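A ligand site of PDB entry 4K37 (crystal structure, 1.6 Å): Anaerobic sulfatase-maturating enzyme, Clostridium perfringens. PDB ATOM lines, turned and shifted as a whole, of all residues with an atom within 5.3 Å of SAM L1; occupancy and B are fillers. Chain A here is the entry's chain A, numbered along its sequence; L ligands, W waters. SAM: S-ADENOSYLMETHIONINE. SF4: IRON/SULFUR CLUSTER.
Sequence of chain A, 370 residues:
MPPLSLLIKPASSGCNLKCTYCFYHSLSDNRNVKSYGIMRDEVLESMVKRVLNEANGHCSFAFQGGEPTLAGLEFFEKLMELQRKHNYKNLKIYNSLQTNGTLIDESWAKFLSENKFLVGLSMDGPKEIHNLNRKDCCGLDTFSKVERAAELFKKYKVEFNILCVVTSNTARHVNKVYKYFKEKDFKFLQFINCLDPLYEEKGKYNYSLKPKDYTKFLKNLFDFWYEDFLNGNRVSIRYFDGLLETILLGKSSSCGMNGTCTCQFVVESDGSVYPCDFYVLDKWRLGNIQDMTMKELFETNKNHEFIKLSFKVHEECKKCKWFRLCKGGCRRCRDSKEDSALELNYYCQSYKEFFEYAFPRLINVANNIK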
ATOM      1  N   CYS A  15      13.949  19.846 -35.224  1.00  0.00           N
ATOM      2  CA  CYS A  15      15.226  19.475 -34.634  1.00  0.00           C
ATOM      3  C   CYS A  15      15.788  18.238 -35.296  1.00  0.00           C
ATOM      4  O   CYS A  15      15.041  17.405 -35.833  1.00  0.00           O
ATOM      5  CB  CYS A  15      15.089  19.243 -33.134  1.00  0.00           C
ATOM      6  SG  CYS A  15      16.704  19.200 -32.299  1.00  0.00           S
ATOM      7  N   TYR A  21      14.267  13.627 -22.813  1.00  0.00           N
ATOM      8  CA  TYR A  21      13.461  14.423 -21.901  1.00  0.00           C
ATOM      9  C   TYR A  21      12.843  15.642 -22.589  1.00  0.00           C
ATOM     10  O   TYR A  21      12.108  16.385 -21.961  1.00  0.00           O
ATOM     11  CB  TYR A  21      14.317  14.893 -20.702  1.00  0.00           C
ATOM     12  CG  TYR A  21      15.665  15.465 -21.094  1.00  0.00           C
ATOM     13  CD1 TYR A  21      15.756  16.631 -21.853  1.00  0.00           C
ATOM     14  CD2 TYR A  21      16.839  14.837 -20.713  1.00  0.00           C
ATOM     15  CE1 TYR A  21      17.002  17.145 -22.217  1.00  0.00           C
ATOM     16  CE2 TYR A  21      18.068  15.327 -21.055  1.00  0.00           C
ATOM     17  CZ  TYR A  21      18.148  16.489 -21.822  1.00  0.00           C
ATOM     18  OH  TYR A  21      19.382  16.970 -22.165  1.00  0.00           O
ATOM     19  N   CYS A  22      13.118  15.841 -23.874  1.00  0.00           N
ATOM     20  CA  CYS A  22      12.770  17.119 -24.482  1.00  0.00           C
ATOM     21  C   CYS A  22      11.324  17.178 -24.963  1.00  0.00           C
ATOM     22  O   CYS A  22      10.884  16.340 -25.739  1.00  0.00           O
ATOM     23  CB  CYS A  22      13.706  17.435 -25.643  1.00  0.00           C
ATOM     24  SG  CYS A  22      13.298  18.982 -26.479  1.00  0.00           S
ATOM     25  N   PHE A  23      10.604  18.197 -24.506  1.00  0.00           N
ATOM     26  CA  PHE A  23       9.235  18.418 -24.962  1.00  0.00           C
ATOM     27  C   PHE A  23       9.115  19.610 -25.921  1.00  0.00           C
ATOM     28  O   PHE A  23       8.023  20.073 -26.217  1.00  0.00           O
ATOM     29  CB  PHE A  23       8.283  18.587 -23.759  1.00  0.00           C
ATOM     30  CG  PHE A  23       8.737  19.621 -22.750  1.00  0.00           C
ATOM     31  CD1 PHE A  23       8.720  20.985 -23.054  1.00  0.00           C
ATOM     32  CD2 PHE A  23       9.176  19.228 -21.494  1.00  0.00           C
ATOM     33  CE1 PHE A  23       9.127  21.929 -22.132  1.00  0.00           C
ATOM     34  CE2 PHE A  23       9.584  20.157 -20.552  1.00  0.00           C
ATOM     35  CZ  PHE A  23       9.569  21.513 -20.867  1.00  0.00           C
ATOM     36  N   TYR A  24      10.263  20.095 -26.410  1.00  0.00           N
ATOM     37  CA  TYR A  24      10.280  21.246 -27.307  1.00  0.00           C
ATOM     38  C   TYR A  24      10.270  20.851 -28.782  1.00  0.00           C
ATOM     39  O   TYR A  24       9.894  21.641 -29.628  1.00  0.00           O
ATOM     40  CB  TYR A  24      11.535  22.085 -27.071  1.00  0.00           C
ATOM     41  CG  TYR A  24      11.629  22.772 -25.719  1.00  0.00           C
ATOM     42  CD1 TYR A  24      12.228  22.137 -24.634  1.00  0.00           C
ATOM     43  CD2 TYR A  24      11.159  24.061 -25.554  1.00  0.00           C
ATOM     44  CE1 TYR A  24      12.348  22.801 -23.402  1.00  0.00           C
ATOM     45  CE2 TYR A  24      11.264  24.722 -24.350  1.00  0.00           C
ATOM     46  CZ  TYR A  24      11.855  24.097 -23.283  1.00  0.00           C
ATOM     47  OH  TYR A  24      11.953  24.781 -22.106  1.00  0.00           O
ATOM     48  N   GLN A  64      16.425  30.185 -30.474  1.00  0.00           N
ATOM     49  CA  GLN A  64      16.275  28.889 -29.803  1.00  0.00           C
ATOM     50  C   GLN A  64      15.363  27.987 -30.637  1.00  0.00           C
ATOM     51  O   GLN A  64      15.335  28.101 -31.873  1.00  0.00           O
ATOM     52  CB  GLN A  64      15.789  29.109 -28.347  1.00  0.00           C
ATOM     53  CG  GLN A  64      16.696  30.079 -27.589  1.00  0.00           C
ATOM     54  CD  GLN A  64      16.263  30.372 -26.130  1.00  0.00           C
ATOM     55  OE1 GLN A  64      15.331  29.763 -25.591  1.00  0.00           O
ATOM     56  NE2 GLN A  64      16.976  31.297 -25.498  1.00  0.00           N
ATOM     57  N   GLY A  65      14.605  27.097 -29.988  1.00  0.00           N
ATOM     58  CA  GLY A  65      13.767  26.143 -30.697  1.00  0.00           C
ATOM     59  C   GLY A  65      13.435  24.918 -29.851  1.00  0.00           C
ATOM     60  O   GLY A  65      13.206  25.037 -28.629  1.00  0.00           O
ATOM     61  N   GLY A  66      13.450  23.728 -30.457  1.00  0.00           N
ATOM     62  CA  GLY A  66      13.947  23.482 -31.794  1.00  0.00           C
ATOM     63  C   GLY A  66      15.446  23.729 -31.889  1.00  0.00           C
ATOM     64  O   GLY A  66      16.050  24.274 -30.960  1.00  0.00           O
ATOM     65  N   GLU A  67      16.050  23.342 -33.001  1.00  0.00           N
ATOM     66  CA  GLU A  67      17.467  23.590 -33.223  1.00  0.00           C
ATOM     67  C   GLU A  67      17.608  24.740 -34.208  1.00  0.00           C
ATOM     68  O   GLU A  67      17.351  24.569 -35.403  1.00  0.00           O
ATOM     69  CB  GLU A  67      18.171  22.340 -33.773  1.00  0.00           C
ATOM     70  CG  GLU A  67      19.615  22.602 -34.194  1.00  0.00           C
ATOM     71  CD  GLU A  67      20.417  23.338 -33.121  1.00  0.00           C
ATOM     72  OE1 GLU A  67      20.282  23.008 -31.914  1.00  0.00           O
ATOM     73  OE2 GLU A  67      21.173  24.260 -33.491  1.00  0.00           O
ATOM     74  N   PRO A  68      18.025  25.924 -33.724  1.00  0.00           N
ATOM     75  CA  PRO A  68      17.944  27.090 -34.610  1.00  0.00           C
ATOM     76  C   PRO A  68      18.911  27.050 -35.788  1.00  0.00           C
ATOM     77  O   PRO A  68      18.658  27.706 -36.812  1.00  0.00           O
ATOM     78  CB  PRO A  68      18.268  28.274 -33.677  1.00  0.00           C
ATOM     79  CG  PRO A  68      19.060  27.662 -32.538  1.00  0.00           C
ATOM     80  CD  PRO A  68      18.409  26.301 -32.349  1.00  0.00           C
ATOM     81  N   GLN A  98      21.007  29.490 -28.796  1.00  0.00           N
ATOM     82  CA  GLN A  98      21.166  28.255 -28.012  1.00  0.00           C
ATOM     83  C   GLN A  98      21.150  27.103 -28.998  1.00  0.00           C
ATOM     84  O   GLN A  98      20.227  26.988 -29.804  1.00  0.00           O
ATOM     85  CB  GLN A  98      20.043  28.068 -26.979  1.00  0.00           C
ATOM     86  CG  GLN A  98      20.178  29.023 -25.804  1.00  0.00           C
ATOM     87  CD  GLN A  98      19.202  28.770 -24.672  1.00  0.00           C
ATOM     88  OE1 GLN A  98      18.279  27.956 -24.783  1.00  0.00           O
ATOM     89  NE2 GLN A  98      19.404  29.475 -23.568  1.00  0.00           N
ATOM     90  N   THR A  99      22.171  26.254 -28.926  1.00  0.00           N
ATOM     91  CA  THR A  99      22.341  25.229 -29.964  1.00  0.00           C
ATOM     92  C   THR A  99      22.771  23.897 -29.386  1.00  0.00           C
ATOM     93  O   THR A  99      23.520  23.829 -28.432  1.00  0.00           O
ATOM     94  CB  THR A  99      23.372  25.658 -31.025  1.00  0.00           C
ATOM     95  OG1 THR A  99      23.454  24.653 -32.043  1.00  0.00           O
ATOM     96  CG2 THR A  99      24.751  25.841 -30.434  1.00  0.00           C
ATOM     97  N   ASN A 100      22.310  22.822 -30.038  1.00  0.00           N
ATOM     98  CA  ASN A 100      22.809  21.490 -29.721  1.00  0.00           C
ATOM     99  C   ASN A 100      24.230  21.234 -30.249  1.00  0.00           C
ATOM    100  O   ASN A 100      24.876  20.256 -29.890  1.00  0.00           O
ATOM    101  CB  ASN A 100      21.815  20.400 -30.170  1.00  0.00           C
ATOM    102  CG  ASN A 100      21.734  20.219 -31.709  1.00  0.00           C
ATOM    103  OD1 ASN A 100      22.703  20.446 -32.442  1.00  0.00           O
ATOM    104  ND2 ASN A 100      20.575  19.777 -32.188  1.00  0.00           N
ATOM    105  N   GLY A 120      24.807  29.612 -26.200  1.00  0.00           N
ATOM    106  CA  GLY A 120      24.638  28.559 -25.203  1.00  0.00           C
ATOM    107  C   GLY A 120      24.739  27.225 -25.897  1.00  0.00           C
ATOM    108  O   GLY A 120      24.036  26.968 -26.880  1.00  0.00           O
ATOM    109  N   SER A 122      24.474  23.139 -25.520  1.00  0.00           N
ATOM    110  CA  SER A 122      23.905  22.104 -24.643  1.00  0.00           C
ATOM    111  C   SER A 122      24.793  20.882 -24.524  1.00  0.00           C
ATOM    112  O   SER A 122      25.039  20.160 -25.498  1.00  0.00           O
ATOM    113  CB  SER A 122      22.500  21.723 -25.087  1.00  0.00           C
ATOM    114  OG  SER A 122      21.632  22.851 -24.991  1.00  0.00           O
ATOM    115  N   ASP A 124      25.457  17.738 -21.533  1.00  0.00           N
ATOM    116  CA  ASP A 124      24.895  17.190 -20.281  1.00  0.00           C
ATOM    117  C   ASP A 124      25.946  16.609 -19.338  1.00  0.00           C
ATOM    118  O   ASP A 124      25.612  16.161 -18.251  1.00  0.00           O
ATOM    119  CB  ASP A 124      23.806  16.152 -20.584  1.00  0.00           C
ATOM    120  CG  ASP A 124      22.437  16.780 -20.822  1.00  0.00           C
ATOM    121  OD1 ASP A 124      22.339  18.037 -20.809  1.00  0.00           O
ATOM    122  OD2 ASP A 124      21.472  16.016 -21.013  1.00  0.00           O
ATOM    123  N   ARG A 134      20.795  12.383 -24.934  1.00  0.00           N
ATOM    124  CA  ARG A 134      20.904  13.261 -26.093  1.00  0.00           C
ATOM    125  C   ARG A 134      21.343  12.502 -27.335  1.00  0.00           C
ATOM    126  O   ARG A 134      22.541  12.425 -27.653  1.00  0.00           O
ATOM    127  CB  ARG A 134      21.840  14.434 -25.780  1.00  0.00           C
ATOM    128  CG  ARG A 134      21.268  15.286 -24.616  1.00  0.00           C
ATOM    129  CD  ARG A 134      22.047  16.587 -24.396  1.00  0.00           C
ATOM    130  NE  ARG A 134      21.915  17.516 -25.520  1.00  0.00           N
ATOM    131  CZ  ARG A 134      20.928  18.392 -25.640  1.00  0.00           C
ATOM    132  NH1 ARG A 134      19.981  18.484 -24.709  1.00  0.00           N
ATOM    133  NH2 ARG A 134      20.893  19.211 -26.689  1.00  0.00           N
ATOM    134  N   LEU A 163      24.864  24.747 -21.280  1.00  0.00           N
ATOM    135  CA  LEU A 163      23.525  24.446 -20.781  1.00  0.00           C
ATOM    136  C   LEU A 163      23.443  22.943 -20.494  1.00  0.00           C
ATOM    137  O   LEU A 163      23.461  22.128 -21.416  1.00  0.00           O
ATOM    138  CB  LEU A 163      22.505  24.817 -21.865  1.00  0.00           C
ATOM    139  CG  LEU A 163      22.586  26.246 -22.391  1.00  0.00           C
ATOM    140  CD1 LEU A 163      21.613  26.403 -23.549  1.00  0.00           C
ATOM    141  CD2 LEU A 163      22.263  27.214 -21.283  1.00  0.00           C
ATOM    142  N   VAL A 165      21.257  19.934 -18.698  1.00  0.00           N
ATOM    143  CA  VAL A 165      20.006  19.489 -18.083  1.00  0.00           C
ATOM    144  C   VAL A 165      20.307  18.568 -16.891  1.00  0.00           C
ATOM    145  O   VAL A 165      21.164  17.694 -16.979  1.00  0.00           O
ATOM    146  CB  VAL A 165      19.094  18.771 -19.132  1.00  0.00           C
ATOM    147  CG1 VAL A 165      17.898  18.117 -18.459  1.00  0.00           C
ATOM    148  CG2 VAL A 165      18.599  19.825 -20.153  1.00  0.00           C
ATOM    149  N   ILE A 192      20.117  23.257 -15.693  1.00  0.00           N
ATOM    150  CA  ILE A 192      18.678  23.427 -15.861  1.00  0.00           C
ATOM    151  C   ILE A 192      17.916  22.256 -15.249  1.00  0.00           C
ATOM    152  O   ILE A 192      18.108  21.117 -15.674  1.00  0.00           O
ATOM    153  CB  ILE A 192      18.312  23.501 -17.367  1.00  0.00           C
ATOM    154  CG1 ILE A 192      19.175  24.559 -18.079  1.00  0.00           C
ATOM    155  CG2 ILE A 192      16.827  23.774 -17.540  1.00  0.00           C
ATOM    156  CD1 ILE A 192      18.983  24.581 -19.614  1.00  0.00           C
ATOM    157  N   ASN A 193      17.063  22.512 -14.256  1.00  0.00           N
ATOM    158  CA  ASN A 193      16.254  21.401 -13.732  1.00  0.00           C
ATOM    159  C   ASN A 193      15.450  20.701 -14.833  1.00  0.00           C
ATOM    160  O   ASN A 193      14.732  21.344 -15.586  1.00  0.00           O
ATOM    161  CB  ASN A 193      15.367  21.786 -12.530  1.00  0.00           C
ATOM    162  CG  ASN A 193      14.530  23.052 -12.750  1.00  0.00           C
ATOM    163  OD1 ASN A 193      14.305  23.826 -11.818  1.00  0.00           O
ATOM    164  ND2 ASN A 193      14.035  23.240 -13.976  1.00  0.00           N
ATOM    165  N   CYS A 194      15.568  19.379 -14.936  1.00  0.00           N
ATOM    166  CA  CYS A 194      14.805  18.653 -15.955  1.00  0.00           C
ATOM    167  C   CYS A 194      13.300  18.660 -15.628  1.00  0.00           C
ATOM    168  O   CYS A 194      12.883  18.208 -14.564  1.00  0.00           O
ATOM    169  CB  CYS A 194      15.286  17.220 -16.110  1.00  0.00           C
ATOM    170  SG  CYS A 194      14.465  16.318 -17.475  1.00  0.00           S
ATOM    171  N   LEU A 195      12.489  19.213 -16.540  1.00  0.00           N
ATOM    172  CA  LEU A 195      11.054  19.309 -16.325  1.00  0.00           C
ATOM    173  C   LEU A 195      10.350  18.138 -16.953  1.00  0.00           C
ATOM    174  O   LEU A 195      10.679  17.723 -18.071  1.00  0.00           O
ATOM    175  CB  LEU A 195      10.507  20.618 -16.921  1.00  0.00           C
ATOM    176  CG  LEU A 195      11.030  21.940 -16.328  1.00  0.00           C
ATOM    177  CD1 LEU A 195      10.660  23.119 -17.235  1.00  0.00           C
ATOM    178  CD2 LEU A 195      10.486  22.141 -14.933  1.00  0.00           C
ATOM    179  N   ASP A 196       9.379  17.571 -16.240  1.00  0.00           N
ATOM    180  CA  ASP A 196       8.470  16.610 -16.853  1.00  0.00           C
ATOM    181  C   ASP A 196       7.497  17.434 -17.706  1.00  0.00           C
ATOM    182  O   ASP A 196       7.314  18.621 -17.474  1.00  0.00           O
ATOM    183  CB  ASP A 196       7.723  15.815 -15.781  1.00  0.00           C
ATOM    184  CG  ASP A 196       8.664  15.046 -14.878  1.00  0.00           C
ATOM    185  OD1 ASP A 196       9.619  14.421 -15.392  1.00  0.00           O
ATOM    186  OD2 ASP A 196       8.460  15.061 -13.637  1.00  0.00           O
HETATM  187  N   SAM L   1      18.110  22.709 -29.593  1.00  0.00           N
HETATM  188  CA  SAM L   1      18.853  23.692 -28.810  1.00  0.00           C
HETATM  189  C   SAM L   1      19.534  23.025 -27.621  1.00  0.00           C
HETATM  190  O   SAM L   1      19.317  21.836 -27.318  1.00  0.00           O
HETATM  191  OXT SAM L   1      20.319  23.706 -26.947  1.00  0.00           O
HETATM  192  CB  SAM L   1      17.960  24.881 -28.409  1.00  0.00           C
HETATM  193  CG  SAM L   1      16.554  24.512 -27.910  1.00  0.00           C
HETATM  194  SD  SAM L   1      16.575  23.515 -26.387  1.00  0.00           S
HETATM  195  CE  SAM L   1      14.836  23.246 -26.027  1.00  0.00           C
HETATM  196  C5' SAM L   1      17.042  24.716 -25.114  1.00  0.00           C
HETATM  197  C4' SAM L   1      17.479  24.050 -23.802  1.00  0.00           C
HETATM  198  O4' SAM L   1      16.376  23.413 -23.147  1.00  0.00           O
HETATM  199  C3' SAM L   1      18.531  22.954 -23.996  1.00  0.00           C
HETATM  200  O3' SAM L   1      19.593  23.146 -23.082  1.00  0.00           O
HETATM  201  C2' SAM L   1      17.800  21.670 -23.632  1.00  0.00           C
HETATM  202  O2' SAM L   1      18.658  20.629 -23.188  1.00  0.00           O
HETATM  203  C1' SAM L   1      16.821  22.194 -22.586  1.00  0.00           C
HETATM  204  N9  SAM L   1      15.742  21.214 -22.326  1.00  0.00           N
HETATM  205  C8  SAM L   1      15.196  20.312 -23.186  1.00  0.00           C
HETATM  206  N7  SAM L   1      14.237  19.601 -22.525  1.00  0.00           N
HETATM  207  C5  SAM L   1      14.188  20.043 -21.240  1.00  0.00           C
HETATM  208  C6  SAM L   1      13.444  19.675 -20.132  1.00  0.00           C
HETATM  209  N6  SAM L   1      12.540  18.700 -20.174  1.00  0.00           N
HETATM  210  N1  SAM L   1      13.636  20.361 -18.945  1.00  0.00           N
HETATM  211  C2  SAM L   1      14.571  21.364 -18.836  1.00  0.00           C
HETATM  212  N3  SAM L   1      15.312  21.718 -19.943  1.00  0.00           N
HETATM  213  C4  SAM L   1      15.127  21.066 -21.110  1.00  0.00           C
HETATM  214 FE1  SF4 L   2      16.393  19.216 -30.104  1.00  0.00          FE
HETATM  215 FE2  SF4 L   2      17.495  20.863 -28.232  1.00  0.00          FE
HETATM  216 FE3  SF4 L   2      17.530  18.038 -27.925  1.00  0.00          FE
HETATM  217 FE4  SF4 L   2      15.181  19.358 -27.712  1.00  0.00          FE
HETATM  218  S1  SF4 L   2      17.012  19.599 -26.342  1.00  0.00           S
HETATM  219  S2  SF4 L   2      15.560  17.471 -28.937  1.00  0.00           S
HETATM  220  S3  SF4 L   2      15.384  21.056 -29.189  1.00  0.00           S
HETATM  221  S4  SF4 L   2      18.594  19.297 -29.487  1.00  0.00           S
HETATM  222  O   HOH W   1      14.604  26.805 -25.890  1.00  0.00           O
HETATM  223  O   HOH W   2      14.574  24.702 -20.594  1.00  0.00           O
HETATM  224  O   HOH W   3      21.298  20.416 -22.179  1.00  0.00           O
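A nitrogen (N) of SAM L1 sits close to the side-chain carboxylate (OE1) of Glu 67. The guanidinium group of Arg 134 sits close to a sulfur (S1) of SF4 L2, 3.6 Å away. A nitrogen (N1) of SAM L1 sits at hydrogen-bond distance from the backbone NH (N) of Leu 195, 2.9 Å away. The side-chain amide nitrogen of Asn 100 lies close to a sulfur (S4) of SF4 L2 (3.4 Å). OG of Ser 122 is in hydrogen-bond range of OXT of SAM L1 (2.5 Å). The backbone NH (N) of Gly 66 sits close to a sulfur (S3) of SF4 L2 (3.5 Å). The side-chain sulfur (SG) of Cys 15 is bound to an iron atom (FE1) of SF4 L2, at 2.2 Å. SG of Cys 22 is bound to FE4 of SF4 L2 (2.3 Å). A nitrogen (N6) of SAM L1 lies within hydrogen-bond range of the backbone carbonyl oxygen (O) of Leu 195 (3.0 Å). O of Tyr 21 is in hydrogen-bond range of N6 of SAM L1, 3.0 Å away. The backbone carbonyl oxygen (O) of Gly 66 sits close to a nitrogen (N) of SAM L1 (2.9 Å). The guanidinium group of Arg 134 is in hydrogen-bond range of an oxygen (O2') of SAM L1 (2.9 Å).
An iron atom (FE2) of SF4 L2 is bound by an oxygen (O) of SAM L1 (2.3 Å).
The side-chain carboxylate of Asp 124 is in hydrogen-bond range of the side-chain hydroxyl of Tyr 21 (2.6 Å). OE2 of Glu 67 is in hydrogen-bond range of OG1 of Thr 99 (2.7 Å). The backbone NH (N) of Val 165 lies within hydrogen-bond range of the side-chain carboxylate (OD1) of Asp 124, at 3.0 Å. N of Ser 122 is in hydrogen-bond range of O of Thr 99, at 3.1 Å. N of Tyr 24 sits close to SG of Cys 22 (3.2 Å). The side-chain hydroxyl (OH) of Tyr 21 is in hydrogen-bond range of the guanidinium group (NH1) of Arg 134 (3.0 Å). The backbone NH (N) of Asn 100 lies within hydrogen-bond range of the side-chain carboxylate (OE1) of Glu 67 (2.8 Å). N of Thr 99 sits at hydrogen-bond distance from O of Gly 120 (2.9 Å).
Residues that only touch SAM L1: Val 165, Tyr 24, Asn 193, Phe 23, Gln 98, Thr 99, Gly 65, Cys 22, Ile 192, Leu 163, Cys 194 and Asn 100. Within 4 Å of SAM L1: Tyr 21, Cys 22, Phe 23, Tyr 24, Gly 65, Gly 66, Glu 67, Gln 98, Thr 99, Asn 100, Ser 122, Arg 134, Leu 163, Val 165, Ile 192, Asn 193, Cys 194 and Leu 195.
Water W3 lies within hydrogen-bond range of an oxygen (O2') of SAM L1, the backbone carbonyl oxygen (O) of Leu 163, the side-chain carboxylate (OD1) of Asp 124 and the guanidinium group (NH1) of Arg 134. Water W2 lies within hydrogen-bond range of OH of Tyr 24 (3.0 Å) and N3 of SAM L1 (3.1 Å).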
